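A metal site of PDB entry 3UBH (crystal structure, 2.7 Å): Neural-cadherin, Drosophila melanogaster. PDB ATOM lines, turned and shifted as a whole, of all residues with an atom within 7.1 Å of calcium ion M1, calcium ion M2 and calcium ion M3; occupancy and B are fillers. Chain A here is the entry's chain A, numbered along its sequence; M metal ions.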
ATOM      1  N   GLU A 230     -26.996  -4.045  17.533  1.00  0.00           N
ATOM      2  CA  GLU A 230     -27.162  -4.582  18.891  1.00  0.00           C
ATOM      3  C   GLU A 230     -27.967  -3.699  19.847  1.00  0.00           C
ATOM      4  O   GLU A 230     -28.435  -4.178  20.889  1.00  0.00           O
ATOM      5  CB  GLU A 230     -25.787  -4.894  19.514  1.00  0.00           C
ATOM      6  CG  GLU A 230     -24.964  -3.669  19.938  1.00  0.00           C
ATOM      7  CD  GLU A 230     -23.816  -3.988  20.889  1.00  0.00           C
ATOM      8  OE1 GLU A 230     -23.951  -4.917  21.711  1.00  0.00           O
ATOM      9  OE2 GLU A 230     -22.772  -3.306  20.818  1.00  0.00           O
ATOM     10  N   ASN A 231     -28.123  -2.431  19.509  1.00  0.00           N
ATOM     11  CA  ASN A 231     -28.749  -1.493  20.424  1.00  0.00           C
ATOM     12  C   ASN A 231     -30.177  -1.150  20.037  1.00  0.00           C
ATOM     13  O   ASN A 231     -30.764  -0.204  20.580  1.00  0.00           O
ATOM     14  CB  ASN A 231     -27.921  -0.204  20.505  1.00  0.00           C
ATOM     15  CG  ASN A 231     -27.951   0.601  19.213  1.00  0.00           C
ATOM     16  OD1 ASN A 231     -28.281   0.087  18.127  1.00  0.00           O
ATOM     17  ND2 ASN A 231     -27.587   1.873  19.315  1.00  0.00           N
ATOM     18  N   LEU A 280     -30.621  -7.082  22.864  1.00  0.00           N
ATOM     19  CA  LEU A 280     -29.427  -7.751  22.365  1.00  0.00           C
ATOM     20  C   LEU A 280     -28.103  -7.273  23.003  1.00  0.00           C
ATOM     21  O   LEU A 280     -28.052  -6.225  23.649  1.00  0.00           O
ATOM     22  CB  LEU A 280     -29.341  -7.623  20.851  1.00  0.00           C
ATOM     23  CG  LEU A 280     -30.536  -8.105  20.029  1.00  0.00           C
ATOM     24  CD1 LEU A 280     -30.692  -7.217  18.813  1.00  0.00           C
ATOM     25  CD2 LEU A 280     -30.358  -9.563  19.640  1.00  0.00           C
ATOM     26  N   ASP A 281     -27.036  -8.057  22.820  1.00  0.00           N
ATOM     27  CA  ASP A 281     -25.693  -7.706  23.292  1.00  0.00           C
ATOM     28  C   ASP A 281     -24.591  -8.419  22.479  1.00  0.00           C
ATOM     29  O   ASP A 281     -24.329  -9.609  22.689  1.00  0.00           O
ATOM     30  CB  ASP A 281     -25.547  -7.980  24.794  1.00  0.00           C
ATOM     31  CG  ASP A 281     -24.313  -7.318  25.395  1.00  0.00           C
ATOM     32  OD1 ASP A 281     -23.893  -7.759  26.480  1.00  0.00           O
ATOM     33  OD2 ASP A 281     -23.777  -6.365  24.802  1.00  0.00           O
ATOM     34  N   PHE A 282     -23.974  -7.681  21.569  1.00  0.00           N
ATOM     35  CA  PHE A 282     -22.855  -8.157  20.751  1.00  0.00           C
ATOM     36  C   PHE A 282     -21.714  -8.647  21.615  1.00  0.00           C
ATOM     37  O   PHE A 282     -20.927  -9.493  21.190  1.00  0.00           O
ATOM     38  CB  PHE A 282     -22.365  -7.018  19.862  1.00  0.00           C
ATOM     39  CG  PHE A 282     -21.377  -7.419  18.803  1.00  0.00           C
ATOM     40  CD1 PHE A 282     -21.815  -7.869  17.554  1.00  0.00           C
ATOM     41  CD2 PHE A 282     -20.012  -7.301  19.031  1.00  0.00           C
ATOM     42  CE1 PHE A 282     -20.906  -8.213  16.562  1.00  0.00           C
ATOM     43  CE2 PHE A 282     -19.088  -7.651  18.056  1.00  0.00           C
ATOM     44  CZ  PHE A 282     -19.531  -8.112  16.819  1.00  0.00           C
ATOM     45  N   GLU A 283     -21.621  -8.114  22.833  1.00  0.00           N
ATOM     46  CA  GLU A 283     -20.587  -8.485  23.792  1.00  0.00           C
ATOM     47  C   GLU A 283     -20.923  -9.741  24.602  1.00  0.00           C
ATOM     48  O   GLU A 283     -20.087 -10.264  25.339  1.00  0.00           O
ATOM     49  CB  GLU A 283     -20.280  -7.306  24.741  1.00  0.00           C
ATOM     50  CG  GLU A 283     -19.345  -6.259  24.161  1.00  0.00           C
ATOM     51  CD  GLU A 283     -19.971  -5.439  23.032  1.00  0.00           C
ATOM     52  OE1 GLU A 283     -20.987  -4.746  23.279  1.00  0.00           O
ATOM     53  OE2 GLU A 283     -19.445  -5.505  21.897  1.00  0.00           O
ATOM     54  N   ASP A 284     -22.155 -10.236  24.470  1.00  0.00           N
ATOM     55  CA  ASP A 284     -22.569 -11.429  25.203  1.00  0.00           C
ATOM     56  C   ASP A 284     -22.278 -12.690  24.394  1.00  0.00           C
ATOM     57  O   ASP A 284     -22.977 -12.997  23.420  1.00  0.00           O
ATOM     58  CB  ASP A 284     -24.051 -11.348  25.569  1.00  0.00           C
ATOM     59  CG  ASP A 284     -24.444 -12.359  26.619  1.00  0.00           C
ATOM     60  OD1 ASP A 284     -24.058 -13.539  26.498  1.00  0.00           O
ATOM     61  OD2 ASP A 284     -25.159 -11.977  27.569  1.00  0.00           O
ATOM     62  N   THR A 315     -24.829  -6.332  14.678  1.00  0.00           N
ATOM     63  CA  THR A 315     -23.588  -5.552  14.571  1.00  0.00           C
ATOM     64  C   THR A 315     -23.192  -4.864  15.871  1.00  0.00           C
ATOM     65  O   THR A 315     -24.027  -4.524  16.704  1.00  0.00           O
ATOM     66  CB  THR A 315     -23.665  -4.488  13.454  1.00  0.00           C
ATOM     67  OG1 THR A 315     -24.969  -3.882  13.474  1.00  0.00           O
ATOM     68  CG2 THR A 315     -23.417  -5.121  12.086  1.00  0.00           C
ATOM     69  N   ASP A 316     -21.885  -4.678  16.027  1.00  0.00           N
ATOM     70  CA  ASP A 316     -21.290  -4.025  17.188  1.00  0.00           C
ATOM     71  C   ASP A 316     -21.586  -2.514  17.150  1.00  0.00           C
ATOM     72  O   ASP A 316     -21.402  -1.857  16.125  1.00  0.00           O
ATOM     73  CB  ASP A 316     -19.778  -4.301  17.202  1.00  0.00           C
ATOM     74  CG  ASP A 316     -19.020  -3.555  18.316  1.00  0.00           C
ATOM     75  OD1 ASP A 316     -19.542  -3.412  19.441  1.00  0.00           O
ATOM     76  OD2 ASP A 316     -17.877  -3.129  18.055  1.00  0.00           O
ATOM     77  N   VAL A 317     -22.061  -1.976  18.270  1.00  0.00           N
ATOM     78  CA  VAL A 317     -22.065  -0.530  18.471  1.00  0.00           C
ATOM     79  C   VAL A 317     -21.113  -0.210  19.605  1.00  0.00           C
ATOM     80  O   VAL A 317     -20.839  -1.063  20.468  1.00  0.00           O
ATOM     81  CB  VAL A 317     -23.483   0.069  18.738  1.00  0.00           C
ATOM     82  CG1 VAL A 317     -24.500  -0.479  17.721  1.00  0.00           C
ATOM     83  CG2 VAL A 317     -23.941  -0.162  20.185  1.00  0.00           C
ATOM     84  N   ASN A 318     -20.588   1.004  19.603  1.00  0.00           N
ATOM     85  CA  ASN A 318     -19.642   1.431  20.617  1.00  0.00           C
ATOM     86  C   ASN A 318     -20.367   1.737  21.923  1.00  0.00           C
ATOM     87  O   ASN A 318     -20.464   2.897  22.323  1.00  0.00           O
ATOM     88  CB  ASN A 318     -18.831   2.636  20.125  1.00  0.00           C
ATOM     89  CG  ASN A 318     -17.696   2.999  21.059  1.00  0.00           C
ATOM     90  OD1 ASN A 318     -16.939   2.135  21.513  1.00  0.00           O
ATOM     91  ND2 ASN A 318     -17.568   4.295  21.357  1.00  0.00           N
ATOM     92  N   ASP A 319     -20.884   0.704  22.566  1.00  0.00           N
ATOM     93  CA  ASP A 319     -21.591   0.877  23.849  1.00  0.00           C
ATOM     94  C   ASP A 319     -20.679   0.716  25.069  1.00  0.00           C
ATOM     95  O   ASP A 319     -21.134   0.821  26.206  1.00  0.00           O
ATOM     96  CB  ASP A 319     -22.864  -0.008  23.952  1.00  0.00           C
ATOM     97  CG  ASP A 319     -22.607  -1.476  23.615  1.00  0.00           C
ATOM     98  OD1 ASP A 319     -21.469  -1.860  23.302  1.00  0.00           O
ATOM     99  OD2 ASP A 319     -23.585  -2.268  23.640  1.00  0.00           O
ATOM    100  N   ASN A 320     -19.394   0.472  24.844  1.00  0.00           N
ATOM    101  CA  ASN A 320     -18.469   0.295  25.964  1.00  0.00           C
ATOM    102  C   ASN A 320     -17.340   1.305  26.017  1.00  0.00           C
ATOM    103  O   ASN A 320     -16.716   1.615  24.999  1.00  0.00           O
ATOM    104  CB  ASN A 320     -17.945  -1.132  26.001  1.00  0.00           C
ATOM    105  CG  ASN A 320     -18.948  -2.105  26.560  1.00  0.00           C
ATOM    106  OD1 ASN A 320     -19.174  -2.156  27.774  1.00  0.00           O
ATOM    107  ND2 ASN A 320     -19.584  -2.880  25.682  1.00  0.00           N
ATOM    108  N   ALA A 321     -17.079   1.825  27.209  1.00  0.00           N
ATOM    109  CA  ALA A 321     -15.932   2.705  27.424  1.00  0.00           C
ATOM    110  C   ALA A 321     -14.705   1.924  27.896  1.00  0.00           C
ATOM    111  O   ALA A 321     -14.835   0.910  28.601  1.00  0.00           O
ATOM    112  CB  ALA A 321     -16.299   3.805  28.415  1.00  0.00           C
ATOM    113  N   PRO A 322     -13.492   2.366  27.490  1.00  0.00           N
ATOM    114  CA  PRO A 322     -12.272   1.703  27.993  1.00  0.00           C
ATOM    115  C   PRO A 322     -12.238   1.727  29.527  1.00  0.00           C
ATOM    116  O   PRO A 322     -12.535   2.771  30.110  1.00  0.00           O
ATOM    117  CB  PRO A 322     -11.141   2.579  27.428  1.00  0.00           C
ATOM    118  CG  PRO A 322     -11.728   3.235  26.216  1.00  0.00           C
ATOM    119  CD  PRO A 322     -13.170   3.465  26.555  1.00  0.00           C
ATOM    120  N   ASP A 351     -11.283  -2.567  26.625  1.00  0.00           N
ATOM    121  CA  ASP A 351     -12.550  -2.152  26.022  1.00  0.00           C
ATOM    122  C   ASP A 351     -13.265  -3.377  25.448  1.00  0.00           C
ATOM    123  O   ASP A 351     -12.692  -4.101  24.632  1.00  0.00           O
ATOM    124  CB  ASP A 351     -12.286  -1.115  24.920  1.00  0.00           C
ATOM    125  CG  ASP A 351     -13.549  -0.386  24.450  1.00  0.00           C
ATOM    126  OD1 ASP A 351     -14.632  -1.020  24.308  1.00  0.00           O
ATOM    127  OD2 ASP A 351     -13.474   0.837  24.193  1.00  0.00           O
ATOM    128  N   SER A 352     -14.502  -3.581  25.878  1.00  0.00           N
ATOM    129  CA  SER A 352     -15.331  -4.738  25.487  1.00  0.00           C
ATOM    130  C   SER A 352     -15.700  -4.833  24.000  1.00  0.00           C
ATOM    131  O   SER A 352     -15.945  -5.933  23.498  1.00  0.00           O
ATOM    132  CB  SER A 352     -16.641  -4.729  26.271  1.00  0.00           C
ATOM    133  OG  SER A 352     -16.399  -4.877  27.651  1.00  0.00           O
ATOM    134  N   ASP A 353     -15.786  -3.696  23.318  1.00  0.00           N
ATOM    135  CA  ASP A 353     -16.255  -3.632  21.939  1.00  0.00           C
ATOM    136  C   ASP A 353     -15.263  -4.279  20.971  1.00  0.00           C
ATOM    137  O   ASP A 353     -14.278  -4.894  21.401  1.00  0.00           O
ATOM    138  CB  ASP A 353     -16.539  -2.174  21.527  1.00  0.00           C
ATOM    139  CG  ASP A 353     -17.555  -1.504  22.447  1.00  0.00           C
ATOM    140  OD1 ASP A 353     -18.614  -2.104  22.719  1.00  0.00           O
ATOM    141  OD2 ASP A 353     -17.311  -0.360  22.881  1.00  0.00           O
ATOM    142  N   SER A 354     -15.523  -4.169  19.672  1.00  0.00           N
ATOM    143  CA  SER A 354     -14.659  -4.794  18.665  1.00  0.00           C
ATOM    144  C   SER A 354     -14.078  -3.787  17.680  1.00  0.00           C
ATOM    145  O   SER A 354     -14.436  -2.611  17.703  1.00  0.00           O
ATOM    146  CB  SER A 354     -15.415  -5.898  17.968  1.00  0.00           C
ATOM    147  OG  SER A 354     -15.963  -6.751  18.944  1.00  0.00           O
ATOM    148  N   SER A 356     -12.310  -0.958  15.834  1.00  0.00           N
ATOM    149  CA  SER A 356     -11.863   0.348  16.294  1.00  0.00           C
ATOM    150  C   SER A 356     -12.686   0.931  17.446  1.00  0.00           C
ATOM    151  O   SER A 356     -12.248   1.892  18.106  1.00  0.00           O
ATOM    152  CB  SER A 356     -11.778   1.344  15.130  1.00  0.00           C
ATOM    153  OG  SER A 356     -13.048   1.563  14.569  1.00  0.00           O
ATOM    154  N   ASN A 357     -13.857   0.362  17.704  1.00  0.00           N
ATOM    155  CA  ASN A 357     -14.607   0.713  18.924  1.00  0.00           C
ATOM    156  C   ASN A 357     -13.862   0.210  20.159  1.00  0.00           C
ATOM    157  O   ASN A 357     -14.211   0.573  21.283  1.00  0.00           O
ATOM    158  CB  ASN A 357     -16.023   0.141  18.902  1.00  0.00           C
ATOM    159  CG  ASN A 357     -16.920   0.744  17.839  1.00  0.00           C
ATOM    160  OD1 ASN A 357     -16.820   1.920  17.483  1.00  0.00           O
ATOM    161  ND2 ASN A 357     -17.836  -0.061  17.343  1.00  0.00           N
ATOM    162  N   ALA A 358     -12.848  -0.615  19.946  1.00  0.00           N
ATOM    163  CA  ALA A 358     -11.965  -1.120  21.011  1.00  0.00           C
ATOM    164  C   ALA A 358     -10.504  -0.662  20.882  1.00  0.00           C
ATOM    165  O   ALA A 358      -9.648  -1.042  21.685  1.00  0.00           O
ATOM    166  CB  ALA A 358     -12.039  -2.636  21.065  1.00  0.00           C
ATOM    167  N   GLU A 359     -10.210   0.146  19.865  1.00  0.00           N
ATOM    168  CA  GLU A 359      -8.877   0.681  19.649  1.00  0.00           C
ATOM    169  C   GLU A 359      -8.635   1.803  20.658  1.00  0.00           C
ATOM    170  O   GLU A 359      -9.454   2.702  20.795  1.00  0.00           O
ATOM    171  CB  GLU A 359      -8.767   1.235  18.223  1.00  0.00           C
ATOM    172  CG  GLU A 359      -7.352   1.315  17.670  1.00  0.00           C
ATOM    173  CD  GLU A 359      -6.930   0.056  16.938  1.00  0.00           C
ATOM    174  OE1 GLU A 359      -5.719  -0.269  16.995  1.00  0.00           O
ATOM    175  OE2 GLU A 359      -7.786  -0.611  16.316  1.00  0.00           O
ATOM    176  N   ASP A 400     -11.249   5.523  23.128  1.00  0.00           N
ATOM    177  CA  ASP A 400     -11.393   4.621  21.994  1.00  0.00           C
ATOM    178  C   ASP A 400     -11.532   5.375  20.679  1.00  0.00           C
ATOM    179  O   ASP A 400     -11.620   6.604  20.660  1.00  0.00           O
ATOM    180  CB  ASP A 400     -12.529   3.580  22.198  1.00  0.00           C
ATOM    181  CG  ASP A 400     -13.928   4.192  22.129  1.00  0.00           C
ATOM    182  OD1 ASP A 400     -14.178   5.090  21.294  1.00  0.00           O
ATOM    183  OD2 ASP A 400     -14.793   3.754  22.904  1.00  0.00           O
ATOM    184  N   LYS A 401     -11.560   4.628  19.576  1.00  0.00           N
ATOM    185  CA  LYS A 401     -11.707   5.233  18.244  1.00  0.00           C
ATOM    186  C   LYS A 401     -13.118   5.047  17.671  1.00  0.00           C
ATOM    187  O   LYS A 401     -13.306   4.973  16.458  1.00  0.00           O
ATOM    188  CB  LYS A 401     -10.640   4.699  17.283  1.00  0.00           C
ATOM    189  CG  LYS A 401      -9.194   5.011  17.692  1.00  0.00           C
ATOM    190  CD  LYS A 401      -8.229   4.901  16.501  1.00  0.00           C
ATOM    191  CE  LYS A 401      -6.768   4.849  16.939  1.00  0.00           C
ATOM    192  NZ  LYS A 401      -6.370   6.030  17.766  1.00  0.00           N
ATOM    193  N   GLY A 402     -14.106   4.989  18.572  1.00  0.00           N
ATOM    194  CA  GLY A 402     -15.512   4.869  18.167  1.00  0.00           C
ATOM    195  C   GLY A 402     -16.097   6.183  17.692  1.00  0.00           C
ATOM    196  O   GLY A 402     -15.460   7.227  17.775  1.00  0.00           O
ATOM    197  N   PRO A 405     -16.398   8.793  20.190  1.00  0.00           N
ATOM    198  CA  PRO A 405     -15.500   8.055  21.072  1.00  0.00           C
ATOM    199  C   PRO A 405     -15.877   8.139  22.548  1.00  0.00           C
ATOM    200  O   PRO A 405     -16.222   9.208  23.041  1.00  0.00           O
ATOM    201  CB  PRO A 405     -14.135   8.732  20.829  1.00  0.00           C
ATOM    202  CG  PRO A 405     -14.463  10.114  20.434  1.00  0.00           C
ATOM    203  CD  PRO A 405     -15.779  10.045  19.696  1.00  0.00           C
ATOM    204  N   LYS A 406     -15.802   6.997  23.238  1.00  0.00           N
ATOM    205  CA  LYS A 406     -16.039   6.925  24.684  1.00  0.00           C
ATOM    206  C   LYS A 406     -14.703   6.934  25.434  1.00  0.00           C
ATOM    207  O   LYS A 406     -13.693   6.487  24.898  1.00  0.00           O
ATOM    208  CB  LYS A 406     -16.834   5.657  25.034  1.00  0.00           C
ATOM    209  CG  LYS A 406     -18.255   5.630  24.468  1.00  0.00           C
ATOM    210  CD  LYS A 406     -19.248   5.087  25.501  1.00  0.00           C
ATOM    211  CE  LYS A 406     -20.608   4.778  24.902  1.00  0.00           C
ATOM    212  NZ  LYS A 406     -21.262   5.961  24.275  1.00  0.00           N
HETATM  213 CA    CA M   1     -15.521   1.155  23.055  1.00  0.00          CA
HETATM  214 CA    CA M   2     -20.423  -3.164  21.442  1.00  0.00          CA
HETATM  215 CA    CA M   3     -23.342  -4.371  24.161  1.00  0.00          CA
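The side-chain carboxylate of Glu 230 sits close to the backbone NH of Phe 282, 2.8 Å away.
The backbone carbonyl oxygen of Thr 315 lies within hydrogen-bond range of the backbone NH of Glu 230, 3.1 Å away.
The side-chain carboxylate (OD2) of Asp 316 sits at hydrogen-bond distance from the backbone NH (N) of Ser 354.
The backbone NH (N) of Gly 402 lies within hydrogen-bond range of the side-chain carboxylate (OD1) of Asp 400 (2.7 Å).
OD1 of Asp 319 sits close to ND2 of Asn 320, 3.2 Å away.
The side-chain carboxylate of Asp 316 sits at hydrogen-bond distance from the side-chain amide nitrogen of Asn 357 (3.1 Å).
OE1 of Glu 283 lies close to ND2 of Asn 320.
The backbone NH of Asp 400 is in hydrogen-bond range of the backbone carbonyl oxygen of Lys 406 (3.2 Å).
Four residues have an atom within 4 Å of calcium ion M3: Glu 230, Asp 281, Glu 283 and Asp 319.
O of Asn 357 is bound to calcium ion M1 (2.3 Å).
Calcium ion M1 is bound by the side-chain amide oxygen (OD1) of Asn 318 (2.3 Å).
O of Asn 320 is bound to calcium ion M1.
Calcium ion M1 is bound by OD2 of Asp 353 (2.4 Å).
The side-chain carboxylate (OD2) of Asp 351 is bound to calcium ion M1, at 2.4 Å.
OD1 of Asp 351 is bound to calcium ion M1, at 2.7 Å.
Calcium ion M1 is bound by the side-chain carboxylate (OD2) of Asp 400, 2.7 Å away.
Calcium ion M2 is bound by the side-chain carboxylate (OD1) of Asp 316 (2.2 Å), the backbone carbonyl oxygen (O) of Val 317 (2.4 Å), the side-chain carboxylate (OE2) of Glu 230 (2.4 Å), the side-chain carboxylate (OD1) of Asp 353 (2.5 Å), the side-chain carboxylate (OE1) of Glu 283 (2.5 Å), the side-chain carboxylate (OD1) of Asp 319 (2.5 Å) and the side-chain carboxylate (OE2) of Glu 283 (2.6 Å).
Calcium ion M2 has seven donor atoms within binding distance.
Calcium ion M3 is bound by OD2 of Asp 281 (2.1 Å), OD2 of Asp 319 (2.2 Å), OE1 of Glu 283 (2.5 Å) and OE1 of Glu 230 (2.6 Å).
Calcium ion M3 has four donor atoms within binding distance.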
